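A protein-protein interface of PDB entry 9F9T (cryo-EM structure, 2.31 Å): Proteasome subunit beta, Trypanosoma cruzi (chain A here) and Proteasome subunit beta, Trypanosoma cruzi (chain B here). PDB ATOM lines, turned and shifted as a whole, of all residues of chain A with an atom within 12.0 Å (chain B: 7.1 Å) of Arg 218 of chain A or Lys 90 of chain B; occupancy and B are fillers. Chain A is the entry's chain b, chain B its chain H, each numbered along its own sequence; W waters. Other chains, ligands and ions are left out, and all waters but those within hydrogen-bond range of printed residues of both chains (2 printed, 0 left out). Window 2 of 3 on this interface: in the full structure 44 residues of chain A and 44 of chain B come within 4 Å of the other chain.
The chain-end carboxylate of Arg 218 of chain A is in salt-bridge range of the side-chain amino group of Lys 90 of chain B, at 3.8 Å.
The backbone NH of Cys 97 of chain B is in hydrogen-bond range of the backbone carbonyl oxygen of Thr 89 of chain B (2.9 Å).
Among the printed residues, pairs that only touch across the chains: Ile 216 of chain A with Glu 111 of chain B (3.5 Å), Ile 217 of chain A with Thr 89 of chain B (3.5 Å), Ile 217 of chain A with Lys 90 of chain B (3.4 Å), Ile 217 of chain A with Ala 110 of chain B (3.7 Å) and Ile 217 of chain A with Glu 111 of chain B (3.8 Å).
Arg 218 of chain A touches just one residue of chain B: Lys 90.
Thr 89 of chain B touches one residue of chain A.
No residue of chain A comes within 4 Å of Leu 91 of chain B.
No residue of chain A comes within 4 Å of Cys 97 of chain B.
Ala 110 of chain B touches just one residue of chain A: Ile 217.
No residue of chain A comes within 4 Å of Ala 114 of chain B.
Of the printed residues of chain A, Glu 111 of chain B touches Ile 216 and Ile 217.
Of the printed residues of chain B, Ile 217 of chain A touches Thr 89, Lys 90, Ala 110 and Glu 111.
Printed residues of chain B within 4 Å of Ile 216 of chain A: Glu 111 (3.5 Å).
The nearest residue of chain B that does not touch Arg 218 of chain A is Glu 118 of chain B (6.5 Å).
Of the 10 printed residues of chain A, 3 touch a printed residue of chain B.
Among the printed residues, no Asp or Glu carboxylate lies within 4 Å of a Lys or Arg side-chain nitrogen of the other chain.
Water W2 lies within hydrogen-bond range of OG1 of Thr 89 of chain B, O of Leu 88 of chain B and N of Ile 216 of chain A.
Water W1 bridges O of Ile 217 of chain A (2.7 Å) and N of Lys 90 of chain B (2.8 Å).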
ATOM      1  N   GLY A 208      -2.833  -0.569  -8.144  1.00  0.00           N
ATOM      2  CA  GLY A 208      -4.252  -0.791  -7.811  1.00  0.00           C
ATOM      3  C   GLY A 208      -4.497  -1.892  -6.751  1.00  0.00           C
ATOM      4  O   GLY A 208      -5.615  -1.985  -6.239  1.00  0.00           O
ATOM      5  N   CYS A 210      -2.709  -1.864  -3.899  1.00  0.00           N
ATOM      6  CA  CYS A 210      -2.249  -1.353  -2.638  1.00  0.00           C
ATOM      7  C   CYS A 210      -3.400  -1.171  -1.635  1.00  0.00           C
ATOM      8  O   CYS A 210      -4.552  -1.117  -2.004  1.00  0.00           O
ATOM      9  CB  CYS A 210      -1.551  -0.020  -2.828  1.00  0.00           C
ATOM     10  SG  CYS A 210      -2.710   1.327  -3.165  1.00  0.00           S
ATOM     11  N   PHE A 211      -3.028  -1.057  -0.354  1.00  0.00           N
ATOM     12  CA  PHE A 211      -3.927  -1.038   0.775  1.00  0.00           C
ATOM     13  C   PHE A 211      -4.920   0.121   0.688  1.00  0.00           C
ATOM     14  O   PHE A 211      -6.089  -0.070   0.944  1.00  0.00           O
ATOM     15  CB  PHE A 211      -3.061  -1.001   2.041  1.00  0.00           C
ATOM     16  CG  PHE A 211      -3.754  -1.285   3.338  1.00  0.00           C
ATOM     17  CD1 PHE A 211      -4.545  -0.333   3.942  1.00  0.00           C
ATOM     18  CD2 PHE A 211      -3.613  -2.528   3.952  1.00  0.00           C
ATOM     19  CE1 PHE A 211      -5.142  -0.587   5.166  1.00  0.00           C
ATOM     20  CE2 PHE A 211      -4.224  -2.802   5.170  1.00  0.00           C
ATOM     21  CZ  PHE A 211      -5.008  -1.825   5.771  1.00  0.00           C
ATOM     22  N   GLU A 212      -4.476   1.330   0.398  1.00  0.00           N
ATOM     23  CA  GLU A 212      -5.379   2.458   0.374  1.00  0.00           C
ATOM     24  C   GLU A 212      -6.425   2.320  -0.735  1.00  0.00           C
ATOM     25  O   GLU A 212      -7.604   2.588  -0.518  1.00  0.00           O
ATOM     26  CB  GLU A 212      -4.546   3.739   0.304  1.00  0.00           C
ATOM     27  CG  GLU A 212      -5.296   4.986  -0.168  1.00  0.00           C
ATOM     28  CD  GLU A 212      -4.503   5.805  -1.192  1.00  0.00           C
ATOM     29  OE1 GLU A 212      -3.282   6.045  -0.949  1.00  0.00           O
ATOM     30  OE2 GLU A 212      -5.087   6.188  -2.252  1.00  0.00           O
ATOM     31  N   LYS A 213      -6.054   1.917  -1.948  1.00  0.00           N
ATOM     32  CA  LYS A 213      -7.045   1.840  -3.006  1.00  0.00           C
ATOM     33  C   LYS A 213      -8.038   0.692  -2.806  1.00  0.00           C
ATOM     34  O   LYS A 213      -9.139   0.762  -3.321  1.00  0.00           O
ATOM     35  CB  LYS A 213      -6.387   1.494  -4.336  1.00  0.00           C
ATOM     36  CG  LYS A 213      -5.500   2.552  -4.965  1.00  0.00           C
ATOM     37  CD  LYS A 213      -6.187   3.475  -5.956  1.00  0.00           C
ATOM     38  CE  LYS A 213      -5.196   3.984  -6.979  1.00  0.00           C
ATOM     39  NZ  LYS A 213      -5.606   5.314  -7.463  1.00  0.00           N
ATOM     40  N   THR A 214      -7.669  -0.387  -2.119  1.00  0.00           N
ATOM     41  CA  THR A 214      -8.591  -1.496  -1.980  1.00  0.00           C
ATOM     42  C   THR A 214      -9.410  -1.454  -0.679  1.00  0.00           C
ATOM     43  O   THR A 214     -10.235  -2.359  -0.446  1.00  0.00           O
ATOM     44  CB  THR A 214      -7.833  -2.806  -2.058  1.00  0.00           C
ATOM     45  OG1 THR A 214      -6.833  -2.593  -1.070  1.00  0.00           O
ATOM     46  CG2 THR A 214      -7.166  -2.981  -3.401  1.00  0.00           C
ATOM     47  N   ALA A 215      -9.191  -0.399   0.116  1.00  0.00           N
ATOM     48  CA  ALA A 215      -9.876  -0.187   1.369  1.00  0.00           C
ATOM     49  C   ALA A 215     -11.348   0.071   1.095  1.00  0.00           C
ATOM     50  O   ALA A 215     -11.662   0.799   0.193  1.00  0.00           O
ATOM     51  CB  ALA A 215      -9.267   0.991   2.073  1.00  0.00           C
ATOM     52  N   ILE A 216     -12.226  -0.632   1.803  1.00  0.00           N
ATOM     53  CA  ILE A 216     -13.655  -0.504   1.621  1.00  0.00           C
ATOM     54  C   ILE A 216     -14.183   0.819   2.200  1.00  0.00           C
ATOM     55  O   ILE A 216     -15.155   1.343   1.644  1.00  0.00           O
ATOM     56  CB  ILE A 216     -14.371  -1.692   2.276  1.00  0.00           C
ATOM     57  CG1 ILE A 216     -14.005  -3.036   1.624  1.00  0.00           C
ATOM     58  CG2 ILE A 216     -15.884  -1.458   2.304  1.00  0.00           C
ATOM     59  CD1 ILE A 216     -14.519  -3.151   0.209  1.00  0.00           C
ATOM     60  N   ILE A 217     -13.539   1.347   3.265  1.00  0.00           N
ATOM     61  CA  ILE A 217     -13.958   2.549   3.980  1.00  0.00           C
ATOM     62  C   ILE A 217     -12.762   3.473   4.132  1.00  0.00           C
ATOM     63  O   ILE A 217     -11.753   3.039   4.682  1.00  0.00           O
ATOM     64  CB  ILE A 217     -14.517   2.222   5.389  1.00  0.00           C
ATOM     65  CG1 ILE A 217     -15.749   1.313   5.333  1.00  0.00           C
ATOM     66  CG2 ILE A 217     -14.812   3.485   6.153  1.00  0.00           C
ATOM     67  CD1 ILE A 217     -16.281   0.821   6.674  1.00  0.00           C
ATOM     68  N   ARG A 218     -12.895   4.728   3.659  1.00  0.00           N
ATOM     69  CA  ARG A 218     -11.868   5.760   3.777  1.00  0.00           C
ATOM     70  C   ARG A 218     -12.072   6.559   5.077  1.00  0.00           C
ATOM     71  O   ARG A 218     -11.072   7.167   5.527  1.00  0.00           O
ATOM     72  CB  ARG A 218     -11.856   6.748   2.601  1.00  0.00           C
ATOM     73  CG  ARG A 218     -12.022   6.113   1.227  1.00  0.00           C
ATOM     74  CD  ARG A 218     -11.157   6.698   0.110  1.00  0.00           C
ATOM     75  NE  ARG A 218     -11.672   6.264  -1.193  1.00  0.00           N
ATOM     76  CZ  ARG A 218     -12.663   6.854  -1.867  1.00  0.00           C
ATOM     77  NH1 ARG A 218     -13.267   6.226  -2.862  1.00  0.00           N
ATOM     78  NH2 ARG A 218     -13.077   8.057  -1.510  1.00  0.00           N
ATOM     79  OXT ARG A 218     -13.213   6.549   5.610  1.00  0.00           O
ATOM     80  N   LYS B  87      -9.533  -6.944   3.577  1.00  0.00           N
ATOM     81  CA  LYS B  87     -10.345  -7.526   4.634  1.00  0.00           C
ATOM     82  C   LYS B  87     -10.085  -6.808   5.946  1.00  0.00           C
ATOM     83  O   LYS B  87     -10.802  -7.050   6.875  1.00  0.00           O
ATOM     84  CB  LYS B  87     -10.022  -9.011   4.816  1.00  0.00           C
ATOM     85  CG  LYS B  87     -10.610  -9.897   3.735  1.00  0.00           C
ATOM     86  CD  LYS B  87      -9.908 -11.208   3.598  1.00  0.00           C
ATOM     87  CE  LYS B  87     -10.350 -11.966   2.351  1.00  0.00           C
ATOM     88  NZ  LYS B  87      -9.933 -13.404   2.370  1.00  0.00           N
ATOM     89  N   LEU B  88      -9.109  -5.914   5.980  1.00  0.00           N
ATOM     90  CA  LEU B  88      -8.928  -5.048   7.106  1.00  0.00           C
ATOM     91  C   LEU B  88      -9.621  -3.717   6.881  1.00  0.00           C
ATOM     92  O   LEU B  88      -9.034  -2.817   6.309  1.00  0.00           O
ATOM     93  CB  LEU B  88      -7.454  -4.810   7.346  1.00  0.00           C
ATOM     94  CG  LEU B  88      -6.624  -6.092   7.469  1.00  0.00           C
ATOM     95  CD1 LEU B  88      -5.210  -5.745   7.862  1.00  0.00           C
ATOM     96  CD2 LEU B  88      -7.255  -7.063   8.467  1.00  0.00           C
ATOM     97  N   THR B  89     -10.783  -3.544   7.522  1.00  0.00           N
ATOM     98  CA  THR B  89     -11.644  -2.427   7.256  1.00  0.00           C
ATOM     99  C   THR B  89     -11.538  -1.454   8.403  1.00  0.00           C
ATOM    100  O   THR B  89     -11.498  -1.851   9.529  1.00  0.00           O
ATOM    101  CB  THR B  89     -13.024  -2.993   6.902  1.00  0.00           C
ATOM    102  OG1 THR B  89     -12.845  -3.729   5.687  1.00  0.00           O
ATOM    103  CG2 THR B  89     -14.112  -1.970   6.662  1.00  0.00           C
ATOM    104  N   LYS B  90     -11.477  -0.180   8.095  1.00  0.00           N
ATOM    105  CA  LYS B  90     -11.392   0.872   9.107  1.00  0.00           C
ATOM    106  C   LYS B  90     -12.773   1.216   9.680  1.00  0.00           C
ATOM    107  O   LYS B  90     -13.684   1.334   8.886  1.00  0.00           O
ATOM    108  CB  LYS B  90     -10.719   2.105   8.511  1.00  0.00           C
ATOM    109  CG  LYS B  90     -10.492   3.203   9.530  1.00  0.00           C
ATOM    110  CD  LYS B  90      -9.891   4.505   9.010  1.00  0.00           C
ATOM    111  CE  LYS B  90     -10.923   5.624   8.961  1.00  0.00           C
ATOM    112  NZ  LYS B  90     -10.286   6.936   9.246  1.00  0.00           N
ATOM    113  N   LEU B  91     -12.909   1.311  11.025  1.00  0.00           N
ATOM    114  CA  LEU B  91     -14.142   1.675  11.716  1.00  0.00           C
ATOM    115  C   LEU B  91     -14.011   3.035  12.409  1.00  0.00           C
ATOM    116  O   LEU B  91     -14.993   3.725  12.578  1.00  0.00           O
ATOM    117  CB  LEU B  91     -14.549   0.601  12.734  1.00  0.00           C
ATOM    118  CG  LEU B  91     -14.948  -0.765  12.179  1.00  0.00           C
ATOM    119  CD1 LEU B  91     -15.141  -1.759  13.317  1.00  0.00           C
ATOM    120  CD2 LEU B  91     -16.229  -0.692  11.334  1.00  0.00           C
ATOM    121  N   ALA B  92     -12.823   3.385  12.859  1.00  0.00           N
ATOM    122  CA  ALA B  92     -12.468   4.705  13.378  1.00  0.00           C
ATOM    123  C   ALA B  92     -10.937   4.851  13.314  1.00  0.00           C
ATOM    124  O   ALA B  92     -10.219   3.922  12.943  1.00  0.00           O
ATOM    125  CB  ALA B  92     -12.911   4.853  14.797  1.00  0.00           C
ATOM    126  N   GLU B  93     -10.435   6.012  13.677  1.00  0.00           N
ATOM    127  CA  GLU B  93      -9.030   6.259  13.441  1.00  0.00           C
ATOM    128  C   GLU B  93      -8.228   5.062  13.927  1.00  0.00           C
ATOM    129  O   GLU B  93      -7.335   4.674  13.178  1.00  0.00           O
ATOM    130  CB  GLU B  93      -8.509   7.538  14.097  1.00  0.00           C
ATOM    131  CG  GLU B  93      -7.071   7.841  13.633  1.00  0.00           C
ATOM    132  CD  GLU B  93      -6.309   8.944  14.364  1.00  0.00           C
ATOM    133  OE1 GLU B  93      -6.860   9.516  15.346  1.00  0.00           O
ATOM    134  OE2 GLU B  93      -5.155   9.235  13.959  1.00  0.00           O
ATOM    135  N   LYS B  94      -8.525   4.479  15.118  1.00  0.00           N
ATOM    136  CA  LYS B  94      -7.667   3.409  15.644  1.00  0.00           C
ATOM    137  C   LYS B  94      -8.387   2.098  15.939  1.00  0.00           C
ATOM    138  O   LYS B  94      -7.900   1.275  16.683  1.00  0.00           O
ATOM    139  CB  LYS B  94      -6.912   3.853  16.891  1.00  0.00           C
ATOM    140  CG  LYS B  94      -6.084   5.081  16.664  1.00  0.00           C
ATOM    141  CD  LYS B  94      -4.691   4.863  16.208  1.00  0.00           C
ATOM    142  CE  LYS B  94      -3.937   6.186  16.325  1.00  0.00           C
ATOM    143  NZ  LYS B  94      -3.579   6.514  17.725  1.00  0.00           N
ATOM    144  N   ILE B  95      -9.532   1.949  15.327  1.00  0.00           N
ATOM    145  CA  ILE B  95     -10.283   0.743  15.418  1.00  0.00           C
ATOM    146  C   ILE B  95     -10.517   0.241  14.019  1.00  0.00           C
ATOM    147  O   ILE B  95     -11.024   1.014  13.194  1.00  0.00           O
ATOM    148  CB  ILE B  95     -11.615   1.018  16.123  1.00  0.00           C
ATOM    149  CG1 ILE B  95     -11.393   1.701  17.458  1.00  0.00           C
ATOM    150  CG2 ILE B  95     -12.340  -0.300  16.325  1.00  0.00           C
ATOM    151  CD1 ILE B  95     -12.692   2.150  18.095  1.00  0.00           C
ATOM    152  N   TYR B  96     -10.153  -1.053  13.828  1.00  0.00           N
ATOM    153  CA  TYR B  96     -10.387  -1.779  12.579  1.00  0.00           C
ATOM    154  C   TYR B  96     -11.104  -3.085  12.793  1.00  0.00           C
ATOM    155  O   TYR B  96     -10.983  -3.681  13.837  1.00  0.00           O
ATOM    156  CB  TYR B  96      -9.104  -2.121  11.832  1.00  0.00           C
ATOM    157  CG  TYR B  96      -8.547  -0.951  11.036  1.00  0.00           C
ATOM    158  CD1 TYR B  96      -8.115   0.186  11.675  1.00  0.00           C
ATOM    159  CD2 TYR B  96      -8.465  -1.002   9.638  1.00  0.00           C
ATOM    160  CE1 TYR B  96      -7.638   1.248  10.959  1.00  0.00           C
ATOM    161  CE2 TYR B  96      -7.985   0.080   8.900  1.00  0.00           C
ATOM    162  CZ  TYR B  96      -7.553   1.201   9.580  1.00  0.00           C
ATOM    163  OH  TYR B  96      -7.024   2.279   8.887  1.00  0.00           O
ATOM    164  N   CYS B  97     -11.692  -3.622  11.757  1.00  0.00           N
ATOM    165  CA  CYS B  97     -12.133  -4.967  11.882  1.00  0.00           C
ATOM    166  C   CYS B  97     -11.571  -5.874  10.786  1.00  0.00           C
ATOM    167  O   CYS B  97     -11.198  -5.418   9.731  1.00  0.00           O
ATOM    168  CB  CYS B  97     -13.650  -4.900  11.880  1.00  0.00           C
ATOM    169  SG  CYS B  97     -14.273  -4.459  10.281  1.00  0.00           S
ATOM    170  N   ALA B 110     -19.929  -3.355   8.340  1.00  0.00           N
ATOM    171  CA  ALA B 110     -18.825  -2.545   8.814  1.00  0.00           C
ATOM    172  C   ALA B 110     -19.110  -1.069   8.557  1.00  0.00           C
ATOM    173  O   ALA B 110     -18.680  -0.190   9.346  1.00  0.00           O
ATOM    174  CB  ALA B 110     -17.587  -2.941   8.123  1.00  0.00           C
ATOM    175  N   GLU B 111     -19.809  -0.851   7.418  1.00  0.00           N
ATOM    176  CA  GLU B 111     -20.103   0.486   6.949  1.00  0.00           C
ATOM    177  C   GLU B 111     -21.054   1.099   7.975  1.00  0.00           C
ATOM    178  O   GLU B 111     -20.773   2.115   8.561  1.00  0.00           O
ATOM    179  CB  GLU B 111     -20.694   0.471   5.524  1.00  0.00           C
ATOM    180  CG  GLU B 111     -19.691   0.462   4.348  1.00  0.00           C
ATOM    181  CD  GLU B 111     -20.091  -0.232   3.012  1.00  0.00           C
ATOM    182  OE1 GLU B 111     -21.271  -0.710   2.820  1.00  0.00           O
ATOM    183  OE2 GLU B 111     -19.194  -0.374   2.121  1.00  0.00           O
ATOM    184  N   ALA B 114     -19.475   1.925  11.234  1.00  0.00           N
ATOM    185  CA  ALA B 114     -18.567   3.071  11.143  1.00  0.00           C
ATOM    186  C   ALA B 114     -19.319   4.378  11.160  1.00  0.00           C
ATOM    187  O   ALA B 114     -18.834   5.341  11.740  1.00  0.00           O
ATOM    188  CB  ALA B 114     -17.689   3.004   9.900  1.00  0.00           C
ATOM    189  N   GLU B 118     -18.876   7.349  14.101  1.00  0.00           N
ATOM    190  CA  GLU B 118     -18.458   8.714  13.744  1.00  0.00           C
ATOM    191  C   GLU B 118     -19.412   9.757  14.359  1.00  0.00           C
ATOM    192  O   GLU B 118     -18.920  10.737  14.921  1.00  0.00           O
ATOM    193  CB  GLU B 118     -18.291   8.725  12.221  1.00  0.00           C
ATOM    194  CG  GLU B 118     -18.256  10.057  11.497  1.00  0.00           C
ATOM    195  CD  GLU B 118     -18.240   9.840   9.971  1.00  0.00           C
ATOM    196  OE1 GLU B 118     -19.263   9.318   9.420  1.00  0.00           O
ATOM    197  OE2 GLU B 118     -17.196  10.149   9.319  1.00  0.00           O
ATOM    198  N   ILE B 231      -2.001  -4.480   9.707  1.00  0.00           N
ATOM    199  CA  ILE B 231      -2.006  -3.140  10.243  1.00  0.00           C
ATOM    200  C   ILE B 231      -1.805  -3.176  11.750  1.00  0.00           C
ATOM    201  O   ILE B 231      -2.216  -4.121  12.383  1.00  0.00           O
ATOM    202  CB  ILE B 231      -3.194  -2.318   9.762  1.00  0.00           C
ATOM    203  CG1 ILE B 231      -3.041  -0.890  10.276  1.00  0.00           C
ATOM    204  CG2 ILE B 231      -4.518  -2.881  10.220  1.00  0.00           C
ATOM    205  CD1 ILE B 231      -4.158   0.028   9.815  1.00  0.00           C
HETATM  206  O   HOH W   1     -11.281   0.419   5.357  1.00  0.00           O
HETATM  207  O   HOH W   2     -10.995  -2.989   3.826  1.00  0.00           O
